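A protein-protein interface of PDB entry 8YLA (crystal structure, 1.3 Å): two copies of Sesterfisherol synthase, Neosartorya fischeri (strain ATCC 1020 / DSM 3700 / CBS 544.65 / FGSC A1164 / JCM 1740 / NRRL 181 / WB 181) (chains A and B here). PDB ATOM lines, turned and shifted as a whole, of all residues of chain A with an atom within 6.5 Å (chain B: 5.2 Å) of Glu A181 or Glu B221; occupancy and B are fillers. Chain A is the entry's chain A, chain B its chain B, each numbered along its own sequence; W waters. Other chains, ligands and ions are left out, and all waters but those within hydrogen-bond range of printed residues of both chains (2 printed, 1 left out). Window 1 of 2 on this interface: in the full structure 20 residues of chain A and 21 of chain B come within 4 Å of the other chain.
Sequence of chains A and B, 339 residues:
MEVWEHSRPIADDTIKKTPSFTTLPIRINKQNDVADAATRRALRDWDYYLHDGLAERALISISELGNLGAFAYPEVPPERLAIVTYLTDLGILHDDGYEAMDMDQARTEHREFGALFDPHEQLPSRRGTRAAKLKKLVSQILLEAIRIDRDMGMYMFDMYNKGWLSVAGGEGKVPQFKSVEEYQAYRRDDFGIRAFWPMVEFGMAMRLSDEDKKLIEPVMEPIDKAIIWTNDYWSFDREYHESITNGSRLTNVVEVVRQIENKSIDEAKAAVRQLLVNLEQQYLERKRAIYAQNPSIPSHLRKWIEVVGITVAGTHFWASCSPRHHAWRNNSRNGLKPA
The backbone NH (N) of Val A180 is in hydrogen-bond range of the side-chain carboxylate (OE1) of Glu B221 (3.0 Å).
N of Glu A181 is in hydrogen-bond range of OE2 of Glu B221, at 2.9 Å.
N of Pro B218 sits close to O of Lys A178 (3.2 Å).
The backbone NH of Lys A178 lies within hydrogen-bond range of the side-chain carboxylate of Glu A182 (3.0 Å).
The side-chain hydroxyl (OG) of Ser A179 is in hydrogen-bond range of the backbone NH (N) of Glu A182 (3.1 Å).
The backbone carbonyl oxygen of Pro B218 is in hydrogen-bond range of the guanidinium group of Arg B286, at 2.9 Å.
The side-chain carboxylate (OE1) of Glu B221 is in salt-bridge range of the guanidinium group (NH1) of Arg B286 (2.8 Å).
Lys A178 touches Glu B217.
OE1 of Glu B221 touches CB of Ser A179, 3.2 Å away.
Val A180 touches Arg B286.
Pro B218 touches Ile A260.
Arg B286 touches Ile A260.
Of chain B, only Glu B221 (2.9 Å) comes within 4 Å of Glu A181.
Glu B221 touches just these residues of chain A: Ser A179 (3.2 Å), Val A180 (3.0 Å) and Glu A181 (2.9 Å).
Printed residues of chain B within 4 Å of Ile A260: Pro B218 and Arg B286.
Of the printed residues of chain B, Lys A178 touches Glu B217 and Pro B218.
Printed residues of chain A within 4 Å of Glu B217: Lys A178.
Gln A184 touches none of the printed residues of chain B.
The nearest printed residue of chain A that does not touch Glu B217 is Glu A182 (4.01 Å).
Hydrophobic or aromatic side chains of chain B that line the printed part of chain A: Pro B218.
Among the printed residues, no Asp or Glu carboxylate lies within 4 Å of a Lys or Arg side-chain nitrogen of the other chain.
No position is printed for both chains.
Water W2 bridges O of Ile A260 (2.7 Å) and O of Arg B286 (2.8 Å).
Water W1 bridges the side-chain carboxylate of Glu B217 and the side-chain carboxylate of Glu A182.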
ATOM      1  N   LYS A 178      20.290  27.389  14.853  1.00  0.00           N
ATOM      2  CA  LYS A 178      21.378  26.589  14.310  1.00  0.00           C
ATOM      3  C   LYS A 178      22.149  27.322  13.227  1.00  0.00           C
ATOM      4  O   LYS A 178      23.031  26.727  12.606  1.00  0.00           O
ATOM      5  CB  LYS A 178      20.842  25.254  13.780  1.00  0.00           C
ATOM      6  CG  LYS A 178      20.462  24.273  14.882  1.00  0.00           C
ATOM      7  CD  LYS A 178      21.669  23.752  15.647  1.00  0.00           C
ATOM      8  CE  LYS A 178      21.233  22.731  16.695  1.00  0.00           C
ATOM      9  NZ  LYS A 178      22.316  21.765  17.038  1.00  0.00           N
ATOM     10  N   SER A 179      21.829  28.586  12.971  1.00  0.00           N
ATOM     11  CA  SER A 179      22.536  29.361  11.966  1.00  0.00           C
ATOM     12  C   SER A 179      22.290  30.836  12.233  1.00  0.00           C
ATOM     13  O   SER A 179      21.281  31.216  12.841  1.00  0.00           O
ATOM     14  CB  SER A 179      22.082  28.988  10.547  1.00  0.00           C
ATOM     15  OG  SER A 179      20.743  29.359  10.295  1.00  0.00           O
ATOM     16  N   VAL A 180      23.240  31.659  11.792  1.00  0.00           N
ATOM     17  CA  VAL A 180      23.066  33.101  11.903  1.00  0.00           C
ATOM     18  C   VAL A 180      21.903  33.564  11.028  1.00  0.00           C
ATOM     19  O   VAL A 180      21.138  34.455  11.418  1.00  0.00           O
ATOM     20  CB  VAL A 180      24.386  33.827  11.597  1.00  0.00           C
ATOM     21  CG1 VAL A 180      24.194  35.338  11.630  1.00  0.00           C
ATOM     22  CG2 VAL A 180      25.430  33.426  12.606  1.00  0.00           C
ATOM     23  N   GLU A 181      21.722  32.945   9.856  1.00  0.00           N
ATOM     24  CA  GLU A 181      20.591  33.266   8.991  1.00  0.00           C
ATOM     25  C   GLU A 181      19.262  33.077   9.709  1.00  0.00           C
ATOM     26  O   GLU A 181      18.394  33.961   9.678  1.00  0.00           O
ATOM     27  CB  GLU A 181      20.636  32.396   7.733  1.00  0.00           C
ATOM     28  CG  GLU A 181      19.460  32.624   6.786  1.00  0.00           C
ATOM     29  CD  GLU A 181      19.553  31.775   5.536  1.00  0.00           C
ATOM     30  OE1 GLU A 181      19.777  30.549   5.654  1.00  0.00           O
ATOM     31  OE2 GLU A 181      19.394  32.340   4.433  1.00  0.00           O
ATOM     32  N   GLU A 182      19.056  31.907  10.314  1.00  0.00           N
ATOM     33  CA  GLU A 182      17.817  31.644  11.029  1.00  0.00           C
ATOM     34  C   GLU A 182      17.660  32.604  12.194  1.00  0.00           C
ATOM     35  O   GLU A 182      16.567  33.139  12.423  1.00  0.00           O
ATOM     36  CB  GLU A 182      17.812  30.194  11.530  1.00  0.00           C
ATOM     37  CG  GLU A 182      16.520  29.741  12.212  1.00  0.00           C
ATOM     38  CD  GLU A 182      16.717  28.594  13.218  1.00  0.00           C
ATOM     39  OE1 GLU A 182      17.798  27.947  13.248  1.00  0.00           O
ATOM     40  OE2 GLU A 182      15.755  28.320  13.974  1.00  0.00           O
ATOM     41  N   TYR A 183      18.741  32.826  12.947  1.00  0.00           N
ATOM     42  CA  TYR A 183      18.699  33.778  14.051  1.00  0.00           C
ATOM     43  C   TYR A 183      18.236  35.149  13.581  1.00  0.00           C
ATOM     44  O   TYR A 183      17.340  35.755  14.184  1.00  0.00           O
ATOM     45  CB  TYR A 183      20.068  33.903  14.717  1.00  0.00           C
ATOM     46  CG  TYR A 183      20.090  35.059  15.689  1.00  0.00           C
ATOM     47  CD1 TYR A 183      19.442  34.962  16.906  1.00  0.00           C
ATOM     48  CD2 TYR A 183      20.696  36.260  15.368  1.00  0.00           C
ATOM     49  CE1 TYR A 183      19.420  36.011  17.787  1.00  0.00           C
ATOM     50  CE2 TYR A 183      20.677  37.326  16.250  1.00  0.00           C
ATOM     51  CZ  TYR A 183      20.027  37.188  17.464  1.00  0.00           C
ATOM     52  OH  TYR A 183      19.997  38.225  18.365  1.00  0.00           O
ATOM     53  N   GLN A 184      18.828  35.653  12.496  1.00  0.00           N
ATOM     54  CA  GLN A 184      18.561  37.023  12.093  1.00  0.00           C
ATOM     55  C   GLN A 184      17.120  37.210  11.632  1.00  0.00           C
ATOM     56  O   GLN A 184      16.527  38.274  11.866  1.00  0.00           O
ATOM     57  CB  GLN A 184      19.569  37.475  11.039  1.00  0.00           C
ATOM     58  CG  GLN A 184      19.477  38.968  10.720  1.00  0.00           C
ATOM     59  CD  GLN A 184      19.820  39.878  11.882  1.00  0.00           C
ATOM     60  OE1 GLN A 184      20.167  39.426  12.975  1.00  0.00           O
ATOM     61  NE2 GLN A 184      19.740  41.184  11.638  1.00  0.00           N
ATOM     62  N   ALA A 185      16.537  36.212  10.967  1.00  0.00           N
ATOM     63  CA  ALA A 185      15.134  36.333  10.573  1.00  0.00           C
ATOM     64  C   ALA A 185      14.241  36.495  11.797  1.00  0.00           C
ATOM     65  O   ALA A 185      13.354  37.355  11.829  1.00  0.00           O
ATOM     66  CB  ALA A 185      14.700  35.112   9.757  1.00  0.00           C
ATOM     67  N   TYR A 186      14.478  35.682  12.826  1.00  0.00           N
ATOM     68  CA  TYR A 186      13.726  35.796  14.069  1.00  0.00           C
ATOM     69  C   TYR A 186      14.030  37.108  14.777  1.00  0.00           C
ATOM     70  O   TYR A 186      13.116  37.775  15.300  1.00  0.00           O
ATOM     71  CB  TYR A 186      14.086  34.611  14.964  1.00  0.00           C
ATOM     72  CG  TYR A 186      13.411  34.587  16.314  1.00  0.00           C
ATOM     73  CD1 TYR A 186      13.913  35.312  17.394  1.00  0.00           C
ATOM     74  CD2 TYR A 186      12.290  33.802  16.530  1.00  0.00           C
ATOM     75  CE1 TYR A 186      13.293  35.275  18.640  1.00  0.00           C
ATOM     76  CE2 TYR A 186      11.667  33.761  17.775  1.00  0.00           C
ATOM     77  CZ  TYR A 186      12.183  34.493  18.823  1.00  0.00           C
ATOM     78  OH  TYR A 186      11.599  34.458  20.070  1.00  0.00           O
ATOM     79  N   ILE A 260      27.248  27.520  18.171  1.00  0.00           N
ATOM     80  CA  ILE A 260      27.506  26.819  16.914  1.00  0.00           C
ATOM     81  C   ILE A 260      28.968  26.822  16.497  1.00  0.00           C
ATOM     82  O   ILE A 260      29.337  26.064  15.592  1.00  0.00           O
ATOM     83  CB  ILE A 260      26.560  27.238  15.768  1.00  0.00           C
ATOM     84  CG1 ILE A 260      26.872  28.652  15.274  1.00  0.00           C
ATOM     85  CG2 ILE A 260      25.116  27.116  16.201  1.00  0.00           C
ATOM     86  CD1 ILE A 260      25.979  29.088  14.126  1.00  0.00           C
ATOM     87  N   ILE B 216      22.926  19.423  11.109  1.00  0.00           N
ATOM     88  CA  ILE B 216      23.948  19.879  10.164  1.00  0.00           C
ATOM     89  C   ILE B 216      23.739  21.304   9.670  1.00  0.00           C
ATOM     90  O   ILE B 216      24.615  21.829   8.960  1.00  0.00           O
ATOM     91  CB  ILE B 216      24.075  18.937   8.953  1.00  0.00           C
ATOM     92  CG1 ILE B 216      22.835  19.023   8.066  1.00  0.00           C
ATOM     93  CG2 ILE B 216      24.370  17.510   9.397  1.00  0.00           C
ATOM     94  CD1 ILE B 216      22.982  18.284   6.755  1.00  0.00           C
ATOM     95  N   GLU B 217      22.631  21.951  10.018  1.00  0.00           N
ATOM     96  CA  GLU B 217      22.411  23.334   9.603  1.00  0.00           C
ATOM     97  C   GLU B 217      23.581  24.278   9.853  1.00  0.00           C
ATOM     98  O   GLU B 217      23.870  25.100   8.964  1.00  0.00           O
ATOM     99  CB  GLU B 217      21.104  23.890  10.183  1.00  0.00           C
ATOM    100  CG  GLU B 217      19.894  23.637   9.295  1.00  0.00           C
ATOM    101  CD  GLU B 217      18.589  23.899  10.002  1.00  0.00           C
ATOM    102  OE1 GLU B 217      18.491  24.935  10.695  1.00  0.00           O
ATOM    103  OE2 GLU B 217      17.658  23.082   9.854  1.00  0.00           O
ATOM    104  N   PRO B 218      24.290  24.225  10.984  1.00  0.00           N
ATOM    105  CA  PRO B 218      25.409  25.159  11.166  1.00  0.00           C
ATOM    106  C   PRO B 218      26.538  24.938  10.183  1.00  0.00           C
ATOM    107  O   PRO B 218      27.261  25.893   9.878  1.00  0.00           O
ATOM    108  CB  PRO B 218      25.867  24.926  12.614  1.00  0.00           C
ATOM    109  CG  PRO B 218      24.905  24.001  13.225  1.00  0.00           C
ATOM    110  CD  PRO B 218      24.026  23.422  12.195  1.00  0.00           C
ATOM    111  N   VAL B 219      26.731  23.702   9.718  1.00  0.00           N
ATOM    112  CA  VAL B 219      27.714  23.403   8.678  1.00  0.00           C
ATOM    113  C   VAL B 219      27.208  23.823   7.301  1.00  0.00           C
ATOM    114  O   VAL B 219      27.966  24.362   6.490  1.00  0.00           O
ATOM    115  CB  VAL B 219      28.086  21.909   8.746  1.00  0.00           C
ATOM    116  CG1 VAL B 219      28.529  21.368   7.385  1.00  0.00           C
ATOM    117  CG2 VAL B 219      29.219  21.716   9.727  1.00  0.00           C
ATOM    118  N   MET B 220      25.929  23.586   7.008  1.00  0.00           N
ATOM    119  CA  MET B 220      25.421  23.892   5.683  1.00  0.00           C
ATOM    120  C   MET B 220      25.310  25.391   5.439  1.00  0.00           C
ATOM    121  O   MET B 220      25.319  25.825   4.276  1.00  0.00           O
ATOM    122  CB  MET B 220      24.087  23.214   5.404  1.00  0.00           C
ATOM    123  CG  MET B 220      24.157  21.710   5.566  1.00  0.00           C
ATOM    124  SD  MET B 220      25.362  20.906   4.510  1.00  0.00           S
ATOM    125  CE  MET B 220      24.756  21.236   2.849  1.00  0.00           C
ATOM    126  N   GLU B 221      25.259  26.199   6.497  1.00  0.00           N
ATOM    127  CA  GLU B 221      25.174  27.648   6.313  1.00  0.00           C
ATOM    128  C   GLU B 221      26.371  28.179   5.540  1.00  0.00           C
ATOM    129  O   GLU B 221      26.176  28.752   4.451  1.00  0.00           O
ATOM    130  CB  GLU B 221      24.925  28.365   7.644  1.00  0.00           C
ATOM    131  CG  GLU B 221      24.916  29.875   7.477  1.00  0.00           C
ATOM    132  CD  GLU B 221      24.635  30.648   8.759  1.00  0.00           C
ATOM    133  OE1 GLU B 221      24.989  30.197   9.870  1.00  0.00           O
ATOM    134  OE2 GLU B 221      24.055  31.748   8.645  1.00  0.00           O
ATOM    135  N   PRO B 222      27.617  28.033   6.003  1.00  0.00           N
ATOM    136  CA  PRO B 222      28.745  28.486   5.175  1.00  0.00           C
ATOM    137  C   PRO B 222      28.923  27.665   3.910  1.00  0.00           C
ATOM    138  O   PRO B 222      29.371  28.212   2.890  1.00  0.00           O
ATOM    139  CB  PRO B 222      29.947  28.357   6.117  1.00  0.00           C
ATOM    140  CG  PRO B 222      29.521  27.326   7.131  1.00  0.00           C
ATOM    141  CD  PRO B 222      28.065  27.567   7.330  1.00  0.00           C
ATOM    142  N   ILE B 223      28.628  26.367   3.945  1.00  0.00           N
ATOM    143  CA  ILE B 223      28.852  25.498   2.789  1.00  0.00           C
ATOM    144  C   ILE B 223      28.004  25.933   1.598  1.00  0.00           C
ATOM    145  O   ILE B 223      28.498  25.987   0.464  1.00  0.00           O
ATOM    146  CB  ILE B 223      28.605  24.025   3.166  1.00  0.00           C
ATOM    147  CG1 ILE B 223      29.776  23.460   3.979  1.00  0.00           C
ATOM    148  CG2 ILE B 223      28.285  23.172   1.942  1.00  0.00           C
ATOM    149  CD1 ILE B 223      31.059  23.213   3.197  1.00  0.00           C
ATOM    150  N   ASP B 224      26.719  26.234   1.814  1.00  0.00           N
ATOM    151  CA  ASP B 224      25.869  26.597   0.685  1.00  0.00           C
ATOM    152  C   ASP B 224      26.327  27.900   0.050  1.00  0.00           C
ATOM    153  O   ASP B 224      26.353  28.022  -1.182  1.00  0.00           O
ATOM    154  CB  ASP B 224      24.411  26.725   1.124  1.00  0.00           C
ATOM    155  CG  ASP B 224      23.718  25.390   1.328  1.00  0.00           C
ATOM    156  OD1 ASP B 224      24.269  24.336   0.974  1.00  0.00           O
ATOM    157  OD2 ASP B 224      22.570  25.424   1.835  1.00  0.00           O
ATOM    158  N   LYS B 225      26.671  28.898   0.871  1.00  0.00           N
ATOM    159  CA  LYS B 225      27.184  30.140   0.310  1.00  0.00           C
ATOM    160  C   LYS B 225      28.488  29.889  -0.423  1.00  0.00           C
ATOM    161  O   LYS B 225      28.703  30.396  -1.531  1.00  0.00           O
ATOM    162  CB  LYS B 225      27.376  31.184   1.411  1.00  0.00           C
ATOM    163  CG  LYS B 225      26.068  31.715   1.987  1.00  0.00           C
ATOM    164  CD  LYS B 225      26.337  32.784   3.030  1.00  0.00           C
ATOM    165  CE  LYS B 225      26.744  32.160   4.349  1.00  0.00           C
ATOM    166  NZ  LYS B 225      26.787  33.134   5.470  1.00  0.00           N
ATOM    167  N   ARG B 286      32.519  25.360  12.398  1.00  0.00           N
ATOM    168  CA  ARG B 286      31.198  24.811  12.666  1.00  0.00           C
ATOM    169  C   ARG B 286      31.267  23.292  12.753  1.00  0.00           C
ATOM    170  O   ARG B 286      30.602  22.671  13.594  1.00  0.00           O
ATOM    171  CB  ARG B 286      30.223  25.226  11.550  1.00  0.00           C
ATOM    172  CG  ARG B 286      30.006  26.731  11.357  1.00  0.00           C
ATOM    173  CD  ARG B 286      29.110  27.360  12.419  1.00  0.00           C
ATOM    174  NE  ARG B 286      28.959  28.804  12.218  1.00  0.00           N
ATOM    175  CZ  ARG B 286      28.022  29.365  11.465  1.00  0.00           C
ATOM    176  NH1 ARG B 286      27.177  28.640  10.763  1.00  0.00           N
ATOM    177  NH2 ARG B 286      27.918  30.690  11.444  1.00  0.00           N
HETATM  178  O   HOH W   1      16.416  27.167  10.165  1.00  0.00           O
HETATM  179  O   HOH W   2      28.219  23.830  14.574  1.00  0.00           O
